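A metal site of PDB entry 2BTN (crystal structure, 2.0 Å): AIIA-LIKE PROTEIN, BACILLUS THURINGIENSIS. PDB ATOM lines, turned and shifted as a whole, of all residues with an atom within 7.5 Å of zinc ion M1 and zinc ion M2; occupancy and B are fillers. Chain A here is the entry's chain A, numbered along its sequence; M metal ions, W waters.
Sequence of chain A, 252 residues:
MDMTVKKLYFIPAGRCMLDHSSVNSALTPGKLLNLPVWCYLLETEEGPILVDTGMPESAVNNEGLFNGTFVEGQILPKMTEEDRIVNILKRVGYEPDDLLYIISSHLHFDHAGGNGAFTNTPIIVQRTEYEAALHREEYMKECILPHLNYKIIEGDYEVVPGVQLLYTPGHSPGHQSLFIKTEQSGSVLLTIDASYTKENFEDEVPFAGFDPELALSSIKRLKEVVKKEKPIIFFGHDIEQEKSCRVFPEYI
Of the 25 residues printed, 4 come within 4 Å of zinc ion M1. Along chain A the residues within 4 Å of zinc ion M1 span positions 106 to 193. The nearest printed residue that does not touch zinc ion M1 is His 111 (4.01 Å).
Of the 25 residues printed, 4 come within 4 Å of zinc ion M2. The nearest printed residue that does not touch zinc ion M2 is His 106 (4.4 Å).
Zinc ion M1 is bound by water W2, a ring nitrogen (NE2) of His 171, a ring nitrogen (NE2) of His 106, a ring nitrogen (ND1) of His 108 and the side-chain carboxylate (OD2) of Asp 193. Slightly farther from zinc ion M1 lies water W3 (2.7 Å).
Zinc ion M2 is bound by OD2 of Asp 193 (2.1 Å). NE2 of His 111 is bound to zinc ion M2, at 2.1 Å. NE2 of His 237 is bound to zinc ion M2. Zinc ion M2 is bound by water W2 (2.2 Å). OD1 of Asp 110 is bound to zinc ion M2. Zinc ion M2 is bound by water W1 (2.6 Å). Zinc ion M2 has six donor atoms within binding distance.
The backbone NH (N) of Asp 193 sits at hydrogen-bond distance from a ring nitrogen (NE2) of His 175 (3.0 Å). ND1 of His 111 is in hydrogen-bond range of OD2 of Asp 52, 2.9 Å away. The backbone carbonyl oxygen of Tyr 196 sits at hydrogen-bond distance from the backbone NH of His 237 (2.9 Å). A ring nitrogen (ND1) of His 237 lies within hydrogen-bond range of the backbone carbonyl oxygen of Pro 36 (2.7 Å). A ring nitrogen (ND1) of His 171 sits at hydrogen-bond distance from the backbone carbonyl oxygen (O) of Ala 208, at 3.0 Å. ND1 of His 106 sits at hydrogen-bond distance from OG of Ser 105, 2.9 Å away.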
ATOM      1  N   CYS A  16     -11.391  -0.251  23.994  1.00  0.00           N
ATOM      2  CA  CYS A  16     -10.047   0.149  23.619  1.00  0.00           C
ATOM      3  C   CYS A  16     -10.078   0.874  22.284  1.00  0.00           C
ATOM      4  O   CYS A  16     -10.579   0.343  21.293  1.00  0.00           O
ATOM      5  CB  CYS A  16      -9.143  -1.091  23.538  1.00  0.00           C
ATOM      6  SG  CYS A  16      -7.399  -0.657  23.577  1.00  0.00           S
ATOM      7  N   LEU A  18      -8.212   2.405  19.009  1.00  0.00           N
ATOM      8  CA  LEU A  18      -7.086   2.070  18.120  1.00  0.00           C
ATOM      9  C   LEU A  18      -7.274   2.791  16.808  1.00  0.00           C
ATOM     10  O   LEU A  18      -8.407   3.176  16.483  1.00  0.00           O
ATOM     11  CB  LEU A  18      -7.103   0.575  17.765  1.00  0.00           C
ATOM     12  CG  LEU A  18      -7.060  -0.548  18.776  1.00  0.00           C
ATOM     13  CD1 LEU A  18      -6.716  -1.807  18.040  1.00  0.00           C
ATOM     14  CD2 LEU A  18      -6.002  -0.273  19.816  1.00  0.00           C
ATOM     15  N   LEU A  35     -13.127  -0.113  20.048  1.00  0.00           N
ATOM     16  CA  LEU A  35     -13.434  -1.547  20.025  1.00  0.00           C
ATOM     17  C   LEU A  35     -13.904  -2.088  21.355  1.00  0.00           C
ATOM     18  O   LEU A  35     -13.373  -1.712  22.404  1.00  0.00           O
ATOM     19  CB  LEU A  35     -12.174  -2.336  19.614  1.00  0.00           C
ATOM     20  CG  LEU A  35     -11.458  -1.968  18.312  1.00  0.00           C
ATOM     21  CD1 LEU A  35     -10.159  -2.789  18.192  1.00  0.00           C
ATOM     22  CD2 LEU A  35     -12.356  -2.189  17.127  1.00  0.00           C
ATOM     23  N   PRO A  36     -14.842  -3.039  21.340  1.00  0.00           N
ATOM     24  CA  PRO A  36     -15.284  -3.664  22.583  1.00  0.00           C
ATOM     25  C   PRO A  36     -14.242  -4.671  23.120  1.00  0.00           C
ATOM     26  O   PRO A  36     -13.596  -5.390  22.337  1.00  0.00           O
ATOM     27  CB  PRO A  36     -16.565  -4.401  22.169  1.00  0.00           C
ATOM     28  CG  PRO A  36     -16.293  -4.803  20.709  1.00  0.00           C
ATOM     29  CD  PRO A  36     -15.512  -3.632  20.158  1.00  0.00           C
ATOM     30  N   VAL A  37     -14.093  -4.707  24.430  1.00  0.00           N
ATOM     31  CA  VAL A  37     -13.301  -5.724  25.142  1.00  0.00           C
ATOM     32  C   VAL A  37     -14.262  -6.703  25.816  1.00  0.00           C
ATOM     33  O   VAL A  37     -15.267  -6.295  26.412  1.00  0.00           O
ATOM     34  CB  VAL A  37     -12.307  -5.090  26.157  1.00  0.00           C
ATOM     35  CG1 VAL A  37     -11.513  -6.171  26.936  1.00  0.00           C
ATOM     36  CG2 VAL A  37     -11.294  -4.148  25.434  1.00  0.00           C
ATOM     37  N   TRP A  38     -13.982  -8.006  25.672  1.00  0.00           N
ATOM     38  CA  TRP A  38     -14.850  -9.064  26.167  1.00  0.00           C
ATOM     39  C   TRP A  38     -14.140 -10.003  27.130  1.00  0.00           C
ATOM     40  O   TRP A  38     -12.948 -10.251  27.010  1.00  0.00           O
ATOM     41  CB  TRP A  38     -15.294  -9.956  25.014  1.00  0.00           C
ATOM     42  CG  TRP A  38     -16.194  -9.296  24.013  1.00  0.00           C
ATOM     43  CD1 TRP A  38     -15.856  -8.912  22.734  1.00  0.00           C
ATOM     44  CD2 TRP A  38     -17.565  -8.970  24.186  1.00  0.00           C
ATOM     45  NE1 TRP A  38     -16.946  -8.371  22.103  1.00  0.00           N
ATOM     46  CE2 TRP A  38     -18.012  -8.402  22.967  1.00  0.00           C
ATOM     47  CE3 TRP A  38     -18.481  -9.124  25.243  1.00  0.00           C
ATOM     48  CZ2 TRP A  38     -19.341  -7.972  22.787  1.00  0.00           C
ATOM     49  CZ3 TRP A  38     -19.791  -8.703  25.059  1.00  0.00           C
ATOM     50  CH2 TRP A  38     -20.207  -8.133  23.836  1.00  0.00           C
ATOM     51  N   ASP A  52     -10.535 -15.159  29.520  1.00  0.00           N
ATOM     52  CA  ASP A  52      -9.944 -13.804  29.545  1.00  0.00           C
ATOM     53  C   ASP A  52     -10.332 -12.957  30.764  1.00  0.00           C
ATOM     54  O   ASP A  52     -11.350 -13.241  31.427  1.00  0.00           O
ATOM     55  CB  ASP A  52     -10.148 -13.067  28.216  1.00  0.00           C
ATOM     56  CG  ASP A  52      -9.362 -13.695  27.092  1.00  0.00           C
ATOM     57  OD1 ASP A  52      -8.432 -14.479  27.416  1.00  0.00           O
ATOM     58  OD2 ASP A  52      -9.600 -13.495  25.873  1.00  0.00           O
ATOM     59  N   SER A 105      -6.852 -16.660  26.219  1.00  0.00           N
ATOM     60  CA  SER A 105      -6.766 -16.812  24.765  1.00  0.00           C
ATOM     61  C   SER A 105      -5.370 -16.399  24.319  1.00  0.00           C
ATOM     62  O   SER A 105      -4.785 -17.002  23.432  1.00  0.00           O
ATOM     63  CB  SER A 105      -7.807 -15.935  24.075  1.00  0.00           C
ATOM     64  OG  SER A 105      -7.575 -14.552  24.368  1.00  0.00           O
ATOM     65  N   HIS A 106      -4.847 -15.344  24.971  1.00  0.00           N
ATOM     66  CA  HIS A 106      -3.483 -14.888  24.826  1.00  0.00           C
ATOM     67  C   HIS A 106      -3.180 -13.833  25.913  1.00  0.00           C
ATOM     68  O   HIS A 106      -4.052 -13.501  26.728  1.00  0.00           O
ATOM     69  CB  HIS A 106      -3.191 -14.392  23.402  1.00  0.00           C
ATOM     70  CG  HIS A 106      -4.015 -13.210  22.967  1.00  0.00           C
ATOM     71  ND1 HIS A 106      -5.390 -13.163  23.084  1.00  0.00           N
ATOM     72  CD2 HIS A 106      -3.657 -12.067  22.341  1.00  0.00           C
ATOM     73  CE1 HIS A 106      -5.833 -12.033  22.563  1.00  0.00           C
ATOM     74  NE2 HIS A 106      -4.803 -11.357  22.098  1.00  0.00           N
ATOM     75  N   LEU A 107      -1.945 -13.327  25.950  1.00  0.00           N
ATOM     76  CA  LEU A 107      -1.556 -12.485  27.068  1.00  0.00           C
ATOM     77  C   LEU A 107      -1.426 -10.991  26.718  1.00  0.00           C
ATOM     78  O   LEU A 107      -0.772 -10.227  27.437  1.00  0.00           O
ATOM     79  CB  LEU A 107      -0.320 -13.055  27.796  1.00  0.00           C
ATOM     80  CG  LEU A 107      -0.440 -14.471  28.396  1.00  0.00           C
ATOM     81  CD1 LEU A 107       0.926 -14.947  28.938  1.00  0.00           C
ATOM     82  CD2 LEU A 107      -1.556 -14.565  29.483  1.00  0.00           C
ATOM     83  N   HIS A 108      -2.077 -10.577  25.633  1.00  0.00           N
ATOM     84  CA  HIS A 108      -2.165  -9.135  25.327  1.00  0.00           C
ATOM     85  C   HIS A 108      -2.913  -8.447  26.462  1.00  0.00           C
ATOM     86  O   HIS A 108      -3.695  -9.096  27.164  1.00  0.00           O
ATOM     87  CB  HIS A 108      -2.838  -8.883  23.980  1.00  0.00           C
ATOM     88  CG  HIS A 108      -1.946  -9.192  22.811  1.00  0.00           C
ATOM     89  ND1 HIS A 108      -2.382  -9.156  21.507  1.00  0.00           N
ATOM     90  CD2 HIS A 108      -0.635  -9.529  22.765  1.00  0.00           C
ATOM     91  CE1 HIS A 108      -1.383  -9.450  20.707  1.00  0.00           C
ATOM     92  NE2 HIS A 108      -0.312  -9.687  21.442  1.00  0.00           N
ATOM     93  N   PHE A 109      -2.657  -7.155  26.632  1.00  0.00           N
ATOM     94  CA  PHE A 109      -3.102  -6.428  27.833  1.00  0.00           C
ATOM     95  C   PHE A 109      -4.639  -6.442  28.030  1.00  0.00           C
ATOM     96  O   PHE A 109      -5.108  -6.334  29.165  1.00  0.00           O
ATOM     97  CB  PHE A 109      -2.540  -4.997  27.852  1.00  0.00           C
ATOM     98  CG  PHE A 109      -3.362  -4.026  27.074  1.00  0.00           C
ATOM     99  CD1 PHE A 109      -4.300  -3.205  27.717  1.00  0.00           C
ATOM    100  CD2 PHE A 109      -3.250  -3.952  25.688  1.00  0.00           C
ATOM    101  CE1 PHE A 109      -5.090  -2.310  27.002  1.00  0.00           C
ATOM    102  CE2 PHE A 109      -4.043  -3.084  24.959  1.00  0.00           C
ATOM    103  CZ  PHE A 109      -4.962  -2.260  25.612  1.00  0.00           C
ATOM    104  N   ASP A 110      -5.402  -6.554  26.945  1.00  0.00           N
ATOM    105  CA  ASP A 110      -6.861  -6.503  27.015  1.00  0.00           C
ATOM    106  C   ASP A 110      -7.527  -7.880  27.230  1.00  0.00           C
ATOM    107  O   ASP A 110      -8.772  -7.976  27.274  1.00  0.00           O
ATOM    108  CB  ASP A 110      -7.456  -5.776  25.779  1.00  0.00           C
ATOM    109  CG  ASP A 110      -6.909  -6.327  24.466  1.00  0.00           C
ATOM    110  OD1 ASP A 110      -7.715  -6.539  23.527  1.00  0.00           O
ATOM    111  OD2 ASP A 110      -5.714  -6.603  24.290  1.00  0.00           O
ATOM    112  N   HIS A 111      -6.705  -8.920  27.376  1.00  0.00           N
ATOM    113  CA  HIS A 111      -7.167 -10.300  27.589  1.00  0.00           C
ATOM    114  C   HIS A 111      -6.635 -10.917  28.885  1.00  0.00           C
ATOM    115  O   HIS A 111      -7.277 -11.802  29.411  1.00  0.00           O
ATOM    116  CB  HIS A 111      -6.783 -11.169  26.377  1.00  0.00           C
ATOM    117  CG  HIS A 111      -7.353 -10.654  25.100  1.00  0.00           C
ATOM    118  ND1 HIS A 111      -8.539 -11.120  24.577  1.00  0.00           N
ATOM    119  CD2 HIS A 111      -6.972  -9.637  24.302  1.00  0.00           C
ATOM    120  CE1 HIS A 111      -8.834 -10.438  23.494  1.00  0.00           C
ATOM    121  NE2 HIS A 111      -7.895  -9.531  23.298  1.00  0.00           N
ATOM    122  N   GLU A 129       2.734 -18.792  23.835  1.00  0.00           N
ATOM    123  CA  GLU A 129       2.278 -17.482  24.321  1.00  0.00           C
ATOM    124  C   GLU A 129       3.001 -17.111  25.615  1.00  0.00           C
ATOM    125  O   GLU A 129       3.538 -16.005  25.754  1.00  0.00           O
ATOM    126  CB  GLU A 129       0.763 -17.442  24.562  1.00  0.00           C
ATOM    127  CG  GLU A 129       0.186 -16.049  24.894  1.00  0.00           C
ATOM    128  CD  GLU A 129       0.251 -15.087  23.729  1.00  0.00           C
ATOM    129  OE1 GLU A 129       0.462 -15.549  22.592  1.00  0.00           O
ATOM    130  OE2 GLU A 129       0.112 -13.855  23.958  1.00  0.00           O
ATOM    131  N   HIS A 171      -1.901 -13.928  15.340  1.00  0.00           N
ATOM    132  CA  HIS A 171      -2.197 -12.648  15.968  1.00  0.00           C
ATOM    133  C   HIS A 171      -1.222 -12.410  17.133  1.00  0.00           C
ATOM    134  O   HIS A 171      -0.731 -11.296  17.323  1.00  0.00           O
ATOM    135  CB  HIS A 171      -3.635 -12.554  16.467  1.00  0.00           C
ATOM    136  CG  HIS A 171      -3.892 -11.329  17.279  1.00  0.00           C
ATOM    137  ND1 HIS A 171      -3.983 -10.074  16.707  1.00  0.00           N
ATOM    138  CD2 HIS A 171      -3.977 -11.142  18.611  1.00  0.00           C
ATOM    139  CE1 HIS A 171      -4.164  -9.174  17.652  1.00  0.00           C
ATOM    140  NE2 HIS A 171      -4.145  -9.792  18.818  1.00  0.00           N
ATOM    141  N   SER A 172      -0.962 -13.453  17.914  1.00  0.00           N
ATOM    142  CA  SER A 172       0.123 -13.455  18.893  1.00  0.00           C
ATOM    143  C   SER A 172       0.812 -14.813  18.752  1.00  0.00           C
ATOM    144  O   SER A 172       0.238 -15.752  18.155  1.00  0.00           O
ATOM    145  CB  SER A 172      -0.435 -13.224  20.306  1.00  0.00           C
ATOM    146  OG  SER A 172      -1.230 -14.323  20.740  1.00  0.00           O
ATOM    147  N   HIS A 175      -1.651 -17.588  20.323  1.00  0.00           N
ATOM    148  CA  HIS A 175      -3.064 -17.264  20.428  1.00  0.00           C
ATOM    149  C   HIS A 175      -3.935 -18.519  20.321  1.00  0.00           C
ATOM    150  O   HIS A 175      -3.663 -19.389  19.501  1.00  0.00           O
ATOM    151  CB  HIS A 175      -3.473 -16.250  19.351  1.00  0.00           C
ATOM    152  CG  HIS A 175      -4.904 -15.823  19.479  1.00  0.00           C
ATOM    153  ND1 HIS A 175      -5.945 -16.554  18.952  1.00  0.00           N
ATOM    154  CD2 HIS A 175      -5.463 -14.782  20.129  1.00  0.00           C
ATOM    155  CE1 HIS A 175      -7.087 -15.963  19.248  1.00  0.00           C
ATOM    156  NE2 HIS A 175      -6.824 -14.883  19.966  1.00  0.00           N
ATOM    157  N   ILE A 192     -11.946 -15.091  19.278  1.00  0.00           N
ATOM    158  CA  ILE A 192     -11.135 -14.109  19.983  1.00  0.00           C
ATOM    159  C   ILE A 192     -10.353 -13.313  18.913  1.00  0.00           C
ATOM    160  O   ILE A 192     -10.959 -12.905  17.934  1.00  0.00           O
ATOM    161  CB  ILE A 192     -10.191 -14.732  21.089  1.00  0.00           C
ATOM    162  CG1 ILE A 192     -10.872 -15.911  21.803  1.00  0.00           C
ATOM    163  CG2 ILE A 192      -9.692 -13.629  22.064  1.00  0.00           C
ATOM    164  CD1 ILE A 192     -12.122 -15.564  22.641  1.00  0.00           C
ATOM    165  N   ASP A 193      -9.048 -13.075  19.108  1.00  0.00           N
ATOM    166  CA  ASP A 193      -8.299 -12.223  18.197  1.00  0.00           C
ATOM    167  C   ASP A 193      -7.711 -12.915  16.957  1.00  0.00           C
ATOM    168  O   ASP A 193      -6.979 -12.302  16.207  1.00  0.00           O
ATOM    169  CB  ASP A 193      -7.222 -11.416  18.933  1.00  0.00           C
ATOM    170  CG  ASP A 193      -7.819 -10.339  19.835  1.00  0.00           C
ATOM    171  OD1 ASP A 193      -9.066 -10.347  20.076  1.00  0.00           O
ATOM    172  OD2 ASP A 193      -7.113  -9.435  20.321  1.00  0.00           O
ATOM    173  N   ALA A 194      -8.069 -14.185  16.738  1.00  0.00           N
ATOM    174  CA  ALA A 194      -7.817 -14.833  15.460  1.00  0.00           C
ATOM    175  C   ALA A 194      -8.568 -14.125  14.306  1.00  0.00           C
ATOM    176  O   ALA A 194      -8.193 -14.269  13.152  1.00  0.00           O
ATOM    177  CB  ALA A 194      -8.172 -16.302  15.532  1.00  0.00           C
ATOM    178  N   TYR A 196     -10.660 -10.128  14.363  1.00  0.00           N
ATOM    179  CA  TYR A 196     -11.330  -9.019  15.076  1.00  0.00           C
ATOM    180  C   TYR A 196     -12.777  -8.866  14.624  1.00  0.00           C
ATOM    181  O   TYR A 196     -13.679  -8.665  15.431  1.00  0.00           O
ATOM    182  CB  TYR A 196     -10.611  -7.686  14.790  1.00  0.00           C
ATOM    183  CG  TYR A 196      -9.318  -7.349  15.516  1.00  0.00           C
ATOM    184  CD1 TYR A 196      -8.599  -8.291  16.252  1.00  0.00           C
ATOM    185  CD2 TYR A 196      -8.793  -6.050  15.427  1.00  0.00           C
ATOM    186  CE1 TYR A 196      -7.390  -7.949  16.917  1.00  0.00           C
ATOM    187  CE2 TYR A 196      -7.600  -5.698  16.069  1.00  0.00           C
ATOM    188  CZ  TYR A 196      -6.910  -6.636  16.801  1.00  0.00           C
ATOM    189  OH  TYR A 196      -5.746  -6.244  17.402  1.00  0.00           O
ATOM    190  N   ALA A 208      -4.016  -6.392  12.428  1.00  0.00           N
ATOM    191  CA  ALA A 208      -2.821  -6.326  13.277  1.00  0.00           C
ATOM    192  C   ALA A 208      -2.451  -7.695  13.845  1.00  0.00           C
ATOM    193  O   ALA A 208      -3.325  -8.489  14.225  1.00  0.00           O
ATOM    194  CB  ALA A 208      -3.008  -5.310  14.403  1.00  0.00           C
ATOM    195  N   GLY A 236     -13.586 -11.224  17.749  1.00  0.00           N
ATOM    196  CA  GLY A 236     -12.939 -10.700  18.944  1.00  0.00           C
ATOM    197  C   GLY A 236     -13.242  -9.249  19.281  1.00  0.00           C
ATOM    198  O   GLY A 236     -13.382  -8.905  20.438  1.00  0.00           O
ATOM    199  N   HIS A 237     -13.326  -8.392  18.271  1.00  0.00           N
ATOM    200  CA  HIS A 237     -13.444  -6.949  18.511  1.00  0.00           C
ATOM    201  C   HIS A 237     -14.342  -6.333  17.439  1.00  0.00           C
ATOM    202  O   HIS A 237     -13.908  -5.496  16.653  1.00  0.00           O
ATOM    203  CB  HIS A 237     -12.057  -6.303  18.485  1.00  0.00           C
ATOM    204  CG  HIS A 237     -11.185  -6.679  19.639  1.00  0.00           C
ATOM    205  ND1 HIS A 237     -11.476  -6.339  20.934  1.00  0.00           N
ATOM    206  CD2 HIS A 237      -9.980  -7.299  19.687  1.00  0.00           C
ATOM    207  CE1 HIS A 237     -10.526  -6.772  21.743  1.00  0.00           C
ATOM    208  NE2 HIS A 237      -9.599  -7.355  20.999  1.00  0.00           N
HETATM  209 ZN    ZN M   1      -4.613  -9.383  20.994  1.00  0.00          ZN
HETATM  210 ZN    ZN M   2      -7.674  -8.045  21.775  1.00  0.00          ZN
HETATM  211  O   HOH W   1      -6.489  -6.167  20.515  1.00  0.00           O
HETATM  212  O   HOH W   2      -5.475  -7.800  22.013  1.00  0.00           O
HETATM  213  O   HOH W   3      -4.836  -7.199  19.468  1.00  0.00           O
